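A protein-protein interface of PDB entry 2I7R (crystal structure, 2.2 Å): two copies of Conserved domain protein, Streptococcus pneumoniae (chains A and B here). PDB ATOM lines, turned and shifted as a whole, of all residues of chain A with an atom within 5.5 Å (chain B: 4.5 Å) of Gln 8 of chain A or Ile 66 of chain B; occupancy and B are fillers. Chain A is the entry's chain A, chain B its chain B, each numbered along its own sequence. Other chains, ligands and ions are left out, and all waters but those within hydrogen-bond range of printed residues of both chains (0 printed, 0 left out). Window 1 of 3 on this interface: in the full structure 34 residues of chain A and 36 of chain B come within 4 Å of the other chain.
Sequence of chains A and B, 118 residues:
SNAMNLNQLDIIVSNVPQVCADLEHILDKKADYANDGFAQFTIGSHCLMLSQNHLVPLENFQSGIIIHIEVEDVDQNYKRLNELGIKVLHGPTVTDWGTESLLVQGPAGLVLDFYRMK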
ATOM      1  N   LEU A   6     -11.767 -10.841  16.371  1.00  0.00           N
ATOM      2  CA  LEU A   6     -12.043 -10.422  17.747  1.00  0.00           C
ATOM      3  C   LEU A   6     -11.022  -9.371  18.149  1.00  0.00           C
ATOM      4  O   LEU A   6      -9.874  -9.691  18.346  1.00  0.00           O
ATOM      5  CB  LEU A   6     -12.012 -11.631  18.708  1.00  0.00           C
ATOM      6  CG  LEU A   6     -12.098 -11.428  20.221  1.00  0.00           C
ATOM      7  CD1 LEU A   6     -13.226 -10.518  20.588  1.00  0.00           C
ATOM      8  CD2 LEU A   6     -12.266 -12.774  20.903  1.00  0.00           C
ATOM      9  N   ASN A   7     -11.506  -8.141  18.309  1.00  0.00           N
ATOM     10  CA  ASN A   7     -10.786  -6.866  18.162  1.00  0.00           C
ATOM     11  C   ASN A   7     -10.860  -6.038  19.433  1.00  0.00           C
ATOM     12  O   ASN A   7      -9.983  -5.241  19.711  1.00  0.00           O
ATOM     13  CB  ASN A   7     -11.525  -5.991  17.101  1.00  0.00           C
ATOM     14  CG  ASN A   7     -10.709  -5.763  15.904  1.00  0.00           C
ATOM     15  OD1 ASN A   7      -9.793  -6.522  15.640  1.00  0.00           O
ATOM     16  ND2 ASN A   7     -11.009  -4.725  15.157  1.00  0.00           N
ATOM     17  N   GLN A   8     -11.992  -6.157  20.118  1.00  0.00           N
ATOM     18  CA  GLN A   8     -12.352  -5.269  21.213  1.00  0.00           C
ATOM     19  C   GLN A   8     -13.171  -6.029  22.251  1.00  0.00           C
ATOM     20  O   GLN A   8     -14.052  -6.818  21.920  1.00  0.00           O
ATOM     21  CB  GLN A   8     -13.162  -4.088  20.665  1.00  0.00           C
ATOM     22  CG  GLN A   8     -13.552  -3.067  21.699  1.00  0.00           C
ATOM     23  CD  GLN A   8     -14.296  -1.856  21.104  1.00  0.00           C
ATOM     24  OE1 GLN A   8     -13.968  -1.379  20.011  1.00  0.00           O
ATOM     25  NE2 GLN A   8     -15.286  -1.349  21.841  1.00  0.00           N
ATOM     26  N   LEU A   9     -12.872  -5.777  23.510  1.00  0.00           N
ATOM     27  CA  LEU A   9     -13.621  -6.365  24.585  1.00  0.00           C
ATOM     28  C   LEU A   9     -14.048  -5.215  25.479  1.00  0.00           C
ATOM     29  O   LEU A   9     -13.222  -4.370  25.847  1.00  0.00           O
ATOM     30  CB  LEU A   9     -12.736  -7.366  25.346  1.00  0.00           C
ATOM     31  CG  LEU A   9     -13.235  -7.892  26.689  1.00  0.00           C
ATOM     32  CD1 LEU A   9     -14.464  -8.821  26.514  1.00  0.00           C
ATOM     33  CD2 LEU A   9     -12.106  -8.596  27.413  1.00  0.00           C
ATOM     34  N   ASP A  10     -15.344  -5.143  25.785  1.00  0.00           N
ATOM     35  CA  ASP A  10     -15.806  -4.153  26.749  1.00  0.00           C
ATOM     36  C   ASP A  10     -16.099  -4.828  28.081  1.00  0.00           C
ATOM     37  O   ASP A  10     -16.684  -5.893  28.115  1.00  0.00           O
ATOM     38  CB  ASP A  10     -17.102  -3.475  26.307  1.00  0.00           C
ATOM     39  CG  ASP A  10     -17.023  -2.847  24.935  1.00  0.00           C
ATOM     40  OD1 ASP A  10     -15.930  -2.762  24.346  1.00  0.00           O
ATOM     41  OD2 ASP A  10     -18.107  -2.455  24.450  1.00  0.00           O
ATOM     42  N   ILE A  11     -15.752  -4.152  29.160  1.00  0.00           N
ATOM     43  CA  ILE A  11     -16.132  -4.542  30.516  1.00  0.00           C
ATOM     44  C   ILE A  11     -17.066  -3.457  31.055  1.00  0.00           C
ATOM     45  O   ILE A  11     -16.703  -2.265  31.084  1.00  0.00           O
ATOM     46  CB  ILE A  11     -14.902  -4.655  31.496  1.00  0.00           C
ATOM     47  CG1 ILE A  11     -13.705  -5.390  30.854  1.00  0.00           C
ATOM     48  CG2 ILE A  11     -15.363  -5.256  32.864  1.00  0.00           C
ATOM     49  CD1 ILE A  11     -14.042  -6.796  30.306  1.00  0.00           C
ATOM     50  N   ILE A  12     -18.252  -3.873  31.487  1.00  0.00           N
ATOM     51  CA  ILE A  12     -19.239  -2.934  32.029  1.00  0.00           C
ATOM     52  C   ILE A  12     -19.022  -2.842  33.551  1.00  0.00           C
ATOM     53  O   ILE A  12     -19.065  -3.874  34.273  1.00  0.00           O
ATOM     54  CB  ILE A  12     -20.667  -3.396  31.743  1.00  0.00           C
ATOM     55  CG1 ILE A  12     -20.875  -3.732  30.273  1.00  0.00           C
ATOM     56  CG2 ILE A  12     -21.686  -2.387  32.251  1.00  0.00           C
ATOM     57  CD1 ILE A  12     -20.215  -2.748  29.316  1.00  0.00           C
ATOM     58  N   HIS A  46      -5.209  -5.445  20.205  1.00  0.00           N
ATOM     59  CA  HIS A  46      -6.557  -5.640  20.778  1.00  0.00           C
ATOM     60  C   HIS A  46      -6.882  -4.420  21.631  1.00  0.00           C
ATOM     61  O   HIS A  46      -5.997  -3.847  22.249  1.00  0.00           O
ATOM     62  CB  HIS A  46      -6.526  -6.926  21.612  1.00  0.00           C
ATOM     63  CG  HIS A  46      -7.855  -7.606  21.813  1.00  0.00           C
ATOM     64  ND1 HIS A  46      -8.937  -6.993  22.417  1.00  0.00           N
ATOM     65  CD2 HIS A  46      -8.244  -8.882  21.559  1.00  0.00           C
ATOM     66  CE1 HIS A  46      -9.939  -7.846  22.495  1.00  0.00           C
ATOM     67  NE2 HIS A  46      -9.544  -9.002  21.990  1.00  0.00           N
ATOM     68  N   CYS A  47      -8.129  -3.977  21.613  1.00  0.00           N
ATOM     69  CA  CYS A  47      -8.571  -2.891  22.498  1.00  0.00           C
ATOM     70  C   CYS A  47      -9.401  -3.429  23.635  1.00  0.00           C
ATOM     71  O   CYS A  47     -10.105  -4.408  23.481  1.00  0.00           O
ATOM     72  CB  CYS A  47      -9.412  -1.868  21.757  1.00  0.00           C
ATOM     73  SG  CYS A  47      -8.451  -0.811  20.748  1.00  0.00           S
ATOM     74  N   LEU A  48      -9.314  -2.772  24.773  1.00  0.00           N
ATOM     75  CA  LEU A  48     -10.114  -3.121  25.925  1.00  0.00           C
ATOM     76  C   LEU A  48     -10.807  -1.837  26.390  1.00  0.00           C
ATOM     77  O   LEU A  48     -10.139  -0.894  26.792  1.00  0.00           O
ATOM     78  CB  LEU A  48      -9.205  -3.745  27.015  1.00  0.00           C
ATOM     79  CG  LEU A  48      -9.722  -4.128  28.423  1.00  0.00           C
ATOM     80  CD1 LEU A  48     -10.669  -5.311  28.400  1.00  0.00           C
ATOM     81  CD2 LEU A  48      -8.551  -4.477  29.326  1.00  0.00           C
ATOM     82  N   MET A  49     -12.136  -1.798  26.332  1.00  0.00           N
ATOM     83  CA  MET A  49     -12.893  -0.663  26.856  1.00  0.00           C
ATOM     84  C   MET A  49     -13.488  -0.929  28.261  1.00  0.00           C
ATOM     85  O   MET A  49     -13.866  -2.061  28.604  1.00  0.00           O
ATOM     86  CB  MET A  49     -14.052  -0.297  25.909  1.00  0.00           C
ATOM     87  CG  MET A  49     -13.668   0.502  24.657  1.00  0.00           C
ATOM     88  SD  MET A  49     -12.085  -0.065  23.673  1.00  0.00           S
ATOM     89  CE  MET A  49     -12.523   0.952  21.958  1.00  0.00           C
ATOM     90  N   LEU A  55     -24.902  -0.683  26.683  1.00  0.00           N
ATOM     91  CA  LEU A  55     -25.203  -0.594  25.263  1.00  0.00           C
ATOM     92  C   LEU A  55     -26.445  -1.440  24.971  1.00  0.00           C
ATOM     93  O   LEU A  55     -27.334  -1.040  24.224  1.00  0.00           O
ATOM     94  CB  LEU A  55     -23.997  -1.022  24.419  1.00  0.00           C
ATOM     95  CG  LEU A  55     -23.972  -0.615  22.942  1.00  0.00           C
ATOM     96  CD1 LEU A  55     -23.942   0.934  22.772  1.00  0.00           C
ATOM     97  CD2 LEU A  55     -22.787  -1.279  22.258  1.00  0.00           C
ATOM     98  N   VAL A  56     -26.509  -2.607  25.595  1.00  0.00           N
ATOM     99  CA  VAL A  56     -27.702  -3.433  25.548  1.00  0.00           C
ATOM    100  C   VAL A  56     -28.041  -3.810  26.992  1.00  0.00           C
ATOM    101  O   VAL A  56     -27.248  -3.526  27.899  1.00  0.00           O
ATOM    102  CB  VAL A  56     -27.536  -4.694  24.661  1.00  0.00           C
ATOM    103  CG1 VAL A  56     -27.230  -4.297  23.245  1.00  0.00           C
ATOM    104  CG2 VAL A  56     -26.481  -5.620  25.220  1.00  0.00           C
ATOM    105  N   LEU A  58     -27.952  -5.586  30.202  1.00  0.00           N
ATOM    106  CA  LEU A  58     -27.033  -6.536  30.863  1.00  0.00           C
ATOM    107  C   LEU A  58     -26.685  -6.004  32.257  1.00  0.00           C
ATOM    108  O   LEU A  58     -27.089  -4.902  32.622  1.00  0.00           O
ATOM    109  CB  LEU A  58     -25.767  -6.797  29.995  1.00  0.00           C
ATOM    110  CG  LEU A  58     -24.957  -5.609  29.434  1.00  0.00           C
ATOM    111  CD1 LEU A  58     -24.621  -4.644  30.517  1.00  0.00           C
ATOM    112  CD2 LEU A  58     -23.683  -6.040  28.711  1.00  0.00           C
ATOM    113  N   ILE B  65     -19.909  -8.105  29.827  1.00  0.00           N
ATOM    114  CA  ILE B  65     -18.925  -7.909  28.739  1.00  0.00           C
ATOM    115  C   ILE B  65     -19.629  -7.912  27.373  1.00  0.00           C
ATOM    116  O   ILE B  65     -20.679  -8.520  27.203  1.00  0.00           O
ATOM    117  CB  ILE B  65     -17.763  -8.990  28.718  1.00  0.00           C
ATOM    118  CG1 ILE B  65     -18.267 -10.359  28.213  1.00  0.00           C
ATOM    119  CG2 ILE B  65     -17.101  -9.098  30.142  1.00  0.00           C
ATOM    120  CD1 ILE B  65     -17.130 -11.430  27.891  1.00  0.00           C
ATOM    121  N   ILE B  66     -19.033  -7.201  26.430  1.00  0.00           N
ATOM    122  CA  ILE B  66     -19.366  -7.323  25.015  1.00  0.00           C
ATOM    123  C   ILE B  66     -18.108  -7.723  24.268  1.00  0.00           C
ATOM    124  O   ILE B  66     -17.074  -7.067  24.395  1.00  0.00           O
ATOM    125  CB  ILE B  66     -19.886  -5.990  24.461  1.00  0.00           C
ATOM    126  CG1 ILE B  66     -21.136  -5.557  25.251  1.00  0.00           C
ATOM    127  CG2 ILE B  66     -20.199  -6.099  23.001  1.00  0.00           C
ATOM    128  CD1 ILE B  66     -21.718  -4.183  24.798  1.00  0.00           C
ATOM    129  N   ILE B  67     -18.193  -8.814  23.514  1.00  0.00           N
ATOM    130  CA  ILE B  67     -17.074  -9.300  22.691  1.00  0.00           C
ATOM    131  C   ILE B  67     -17.358  -8.764  21.299  1.00  0.00           C
ATOM    132  O   ILE B  67     -18.427  -9.080  20.750  1.00  0.00           O
ATOM    133  CB  ILE B  67     -17.097 -10.856  22.556  1.00  0.00           C
ATOM    134  CG1 ILE B  67     -17.106 -11.588  23.903  1.00  0.00           C
ATOM    135  CG2 ILE B  67     -15.972 -11.346  21.680  1.00  0.00           C
ATOM    136  CD1 ILE B  67     -15.959 -11.222  24.742  1.00  0.00           C
ATOM    137  N   HIS B  68     -16.434  -7.983  20.726  1.00  0.00           N
ATOM    138  CA  HIS B  68     -16.650  -7.361  19.413  1.00  0.00           C
ATOM    139  C   HIS B  68     -15.830  -8.045  18.377  1.00  0.00           C
ATOM    140  O   HIS B  68     -14.593  -8.083  18.495  1.00  0.00           O
ATOM    141  CB  HIS B  68     -16.250  -5.876  19.358  1.00  0.00           C
ATOM    142  CG  HIS B  68     -17.033  -4.996  20.257  1.00  0.00           C
ATOM    143  ND1 HIS B  68     -18.119  -4.272  19.826  1.00  0.00           N
ATOM    144  CD2 HIS B  68     -16.902  -4.731  21.575  1.00  0.00           C
ATOM    145  CE1 HIS B  68     -18.629  -3.598  20.842  1.00  0.00           C
ATOM    146  NE2 HIS B  68     -17.897  -3.849  21.914  1.00  0.00           N
ATOM    147  N   LEU B 103     -25.617  -6.255  17.542  1.00  0.00           N
ATOM    148  CA  LEU B 103     -25.496  -6.804  18.888  1.00  0.00           C
ATOM    149  C   LEU B 103     -26.426  -7.986  19.054  1.00  0.00           C
ATOM    150  O   LEU B 103     -27.629  -7.892  18.759  1.00  0.00           O
ATOM    151  CB  LEU B 103     -25.827  -5.743  19.922  1.00  0.00           C
ATOM    152  CG  LEU B 103     -24.643  -4.761  20.006  1.00  0.00           C
ATOM    153  CD1 LEU B 103     -25.113  -3.393  20.351  1.00  0.00           C
ATOM    154  CD2 LEU B 103     -23.583  -5.233  21.013  1.00  0.00           C
ATOM    155  N   VAL B 111     -22.589 -11.341  25.372  1.00  0.00           N
ATOM    156  CA  VAL B 111     -23.117 -10.440  24.333  1.00  0.00           C
ATOM    157  C   VAL B 111     -22.041 -10.297  23.254  1.00  0.00           C
ATOM    158  O   VAL B 111     -20.868 -10.068  23.562  1.00  0.00           O
ATOM    159  CB  VAL B 111     -23.573  -9.048  24.939  1.00  0.00           C
ATOM    160  CG1 VAL B 111     -24.002  -8.087  23.857  1.00  0.00           C
ATOM    161  CG2 VAL B 111     -24.706  -9.252  25.968  1.00  0.00           C
ATOM    162  N   ASP B 113     -20.862  -8.518  19.424  1.00  0.00           N
ATOM    163  CA  ASP B 113     -21.129  -7.455  18.461  1.00  0.00           C
ATOM    164  C   ASP B 113     -20.375  -7.854  17.209  1.00  0.00           C
ATOM    165  O   ASP B 113     -19.189  -8.080  17.285  1.00  0.00           O
ATOM    166  CB  ASP B 113     -20.657  -6.103  19.033  1.00  0.00           C
ATOM    167  CG  ASP B 113     -20.668  -4.949  17.991  1.00  0.00           C
ATOM    168  OD1 ASP B 113     -21.592  -4.877  17.148  1.00  0.00           O
ATOM    169  OD2 ASP B 113     -19.741  -4.113  18.029  1.00  0.00           O
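No position is printed for both chains.
The side-chain carboxylate (OD2) of Asp 10 of chain A sits at hydrogen-bond distance from a ring nitrogen (NE2) of His 68 of chain B (2.9 Å).
O of His 68 of chain B lies within hydrogen-bond range of N of Asn 7 of chain A (3.1 Å).
O of Gln 8 of chain A lies within hydrogen-bond range of N of His 68 of chain B, at 2.9 Å.
O of Ile 66 of chain B is in hydrogen-bond range of N of Asp 10 of chain A, at 2.9 Å.
Among the printed residues, merely in contact across the chains: Leu 6 of chain A with Ile 67 of chain B, Asp 10 of chain A with Ile 65 of chain B, Leu 9 of chain A with Ile 67 of chain B, Leu 6 of chain A with His 68 of chain B, Leu 9 of chain A with Ile 66 of chain B, Leu 55 of chain A with Leu 103 of chain B, Val 56 of chain A with Leu 103 of chain B, Val 56 of chain A with Val 111 of chain B, Ile 11 of chain A with Ile 65 of chain B, Gln 8 of chain A with Ile 67 of chain B, Gln 8 of chain A with Ile 66 of chain B, Leu 55 of chain A with Ile 66 of chain B and Leu 9 of chain A with Ile 65 of chain B.
NE2 of Gln 8 of chain A lies within hydrogen-bond range of OD1 of Asp 10 of chain A.
The backbone carbonyl oxygen (O) of Met 49 of chain A is in hydrogen-bond range of the backbone NH (N) of Ile 11 of chain A (2.9 Å).
O of Asn 7 of chain A is in hydrogen-bond range of N of Cys 47 of chain A (2.9 Å).
OD2 of Asp 113 of chain B is in hydrogen-bond range of ND1 of His 68 of chain B (2.4 Å).
The backbone carbonyl oxygen (O) of Val 111 of chain B lies within hydrogen-bond range of the backbone NH (N) of Ile 67 of chain B (3.0 Å).
The backbone NH of Leu 9 of chain A sits at hydrogen-bond distance from the backbone carbonyl oxygen of Cys 47 of chain A (3.1 Å).
Of chain B, only Ile 66, Ile 67 and His 68 come within 4 Å of Gln 8 of chain A.
Printed residues of chain B within 4 Å of Asp 10 of chain A: Ile 65, Ile 66 and His 68.
Leu 48 of chain A touches none of the printed residues of chain B.
Of chain A, only Gln 8, Leu 9, Asp 10 and Leu 55 come within 4 Å of Ile 66 of chain B.
Printed residues of chain A within 4 Å of Ile 67 of chain B: Leu 6, Gln 8 and Leu 9.
Of the printed residues of chain A, Leu 103 of chain B touches Leu 55 and Val 56.
The nearest residue of chain A that does not touch Ile 66 of chain B is Leu 58 of chain A (4.3 Å).
Among the printed residues, 17 pairs touch across the chains.
Among the printed residues, no Asp or Glu carboxylate lies within 4 Å of a Lys or Arg side-chain nitrogen of the other chain.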
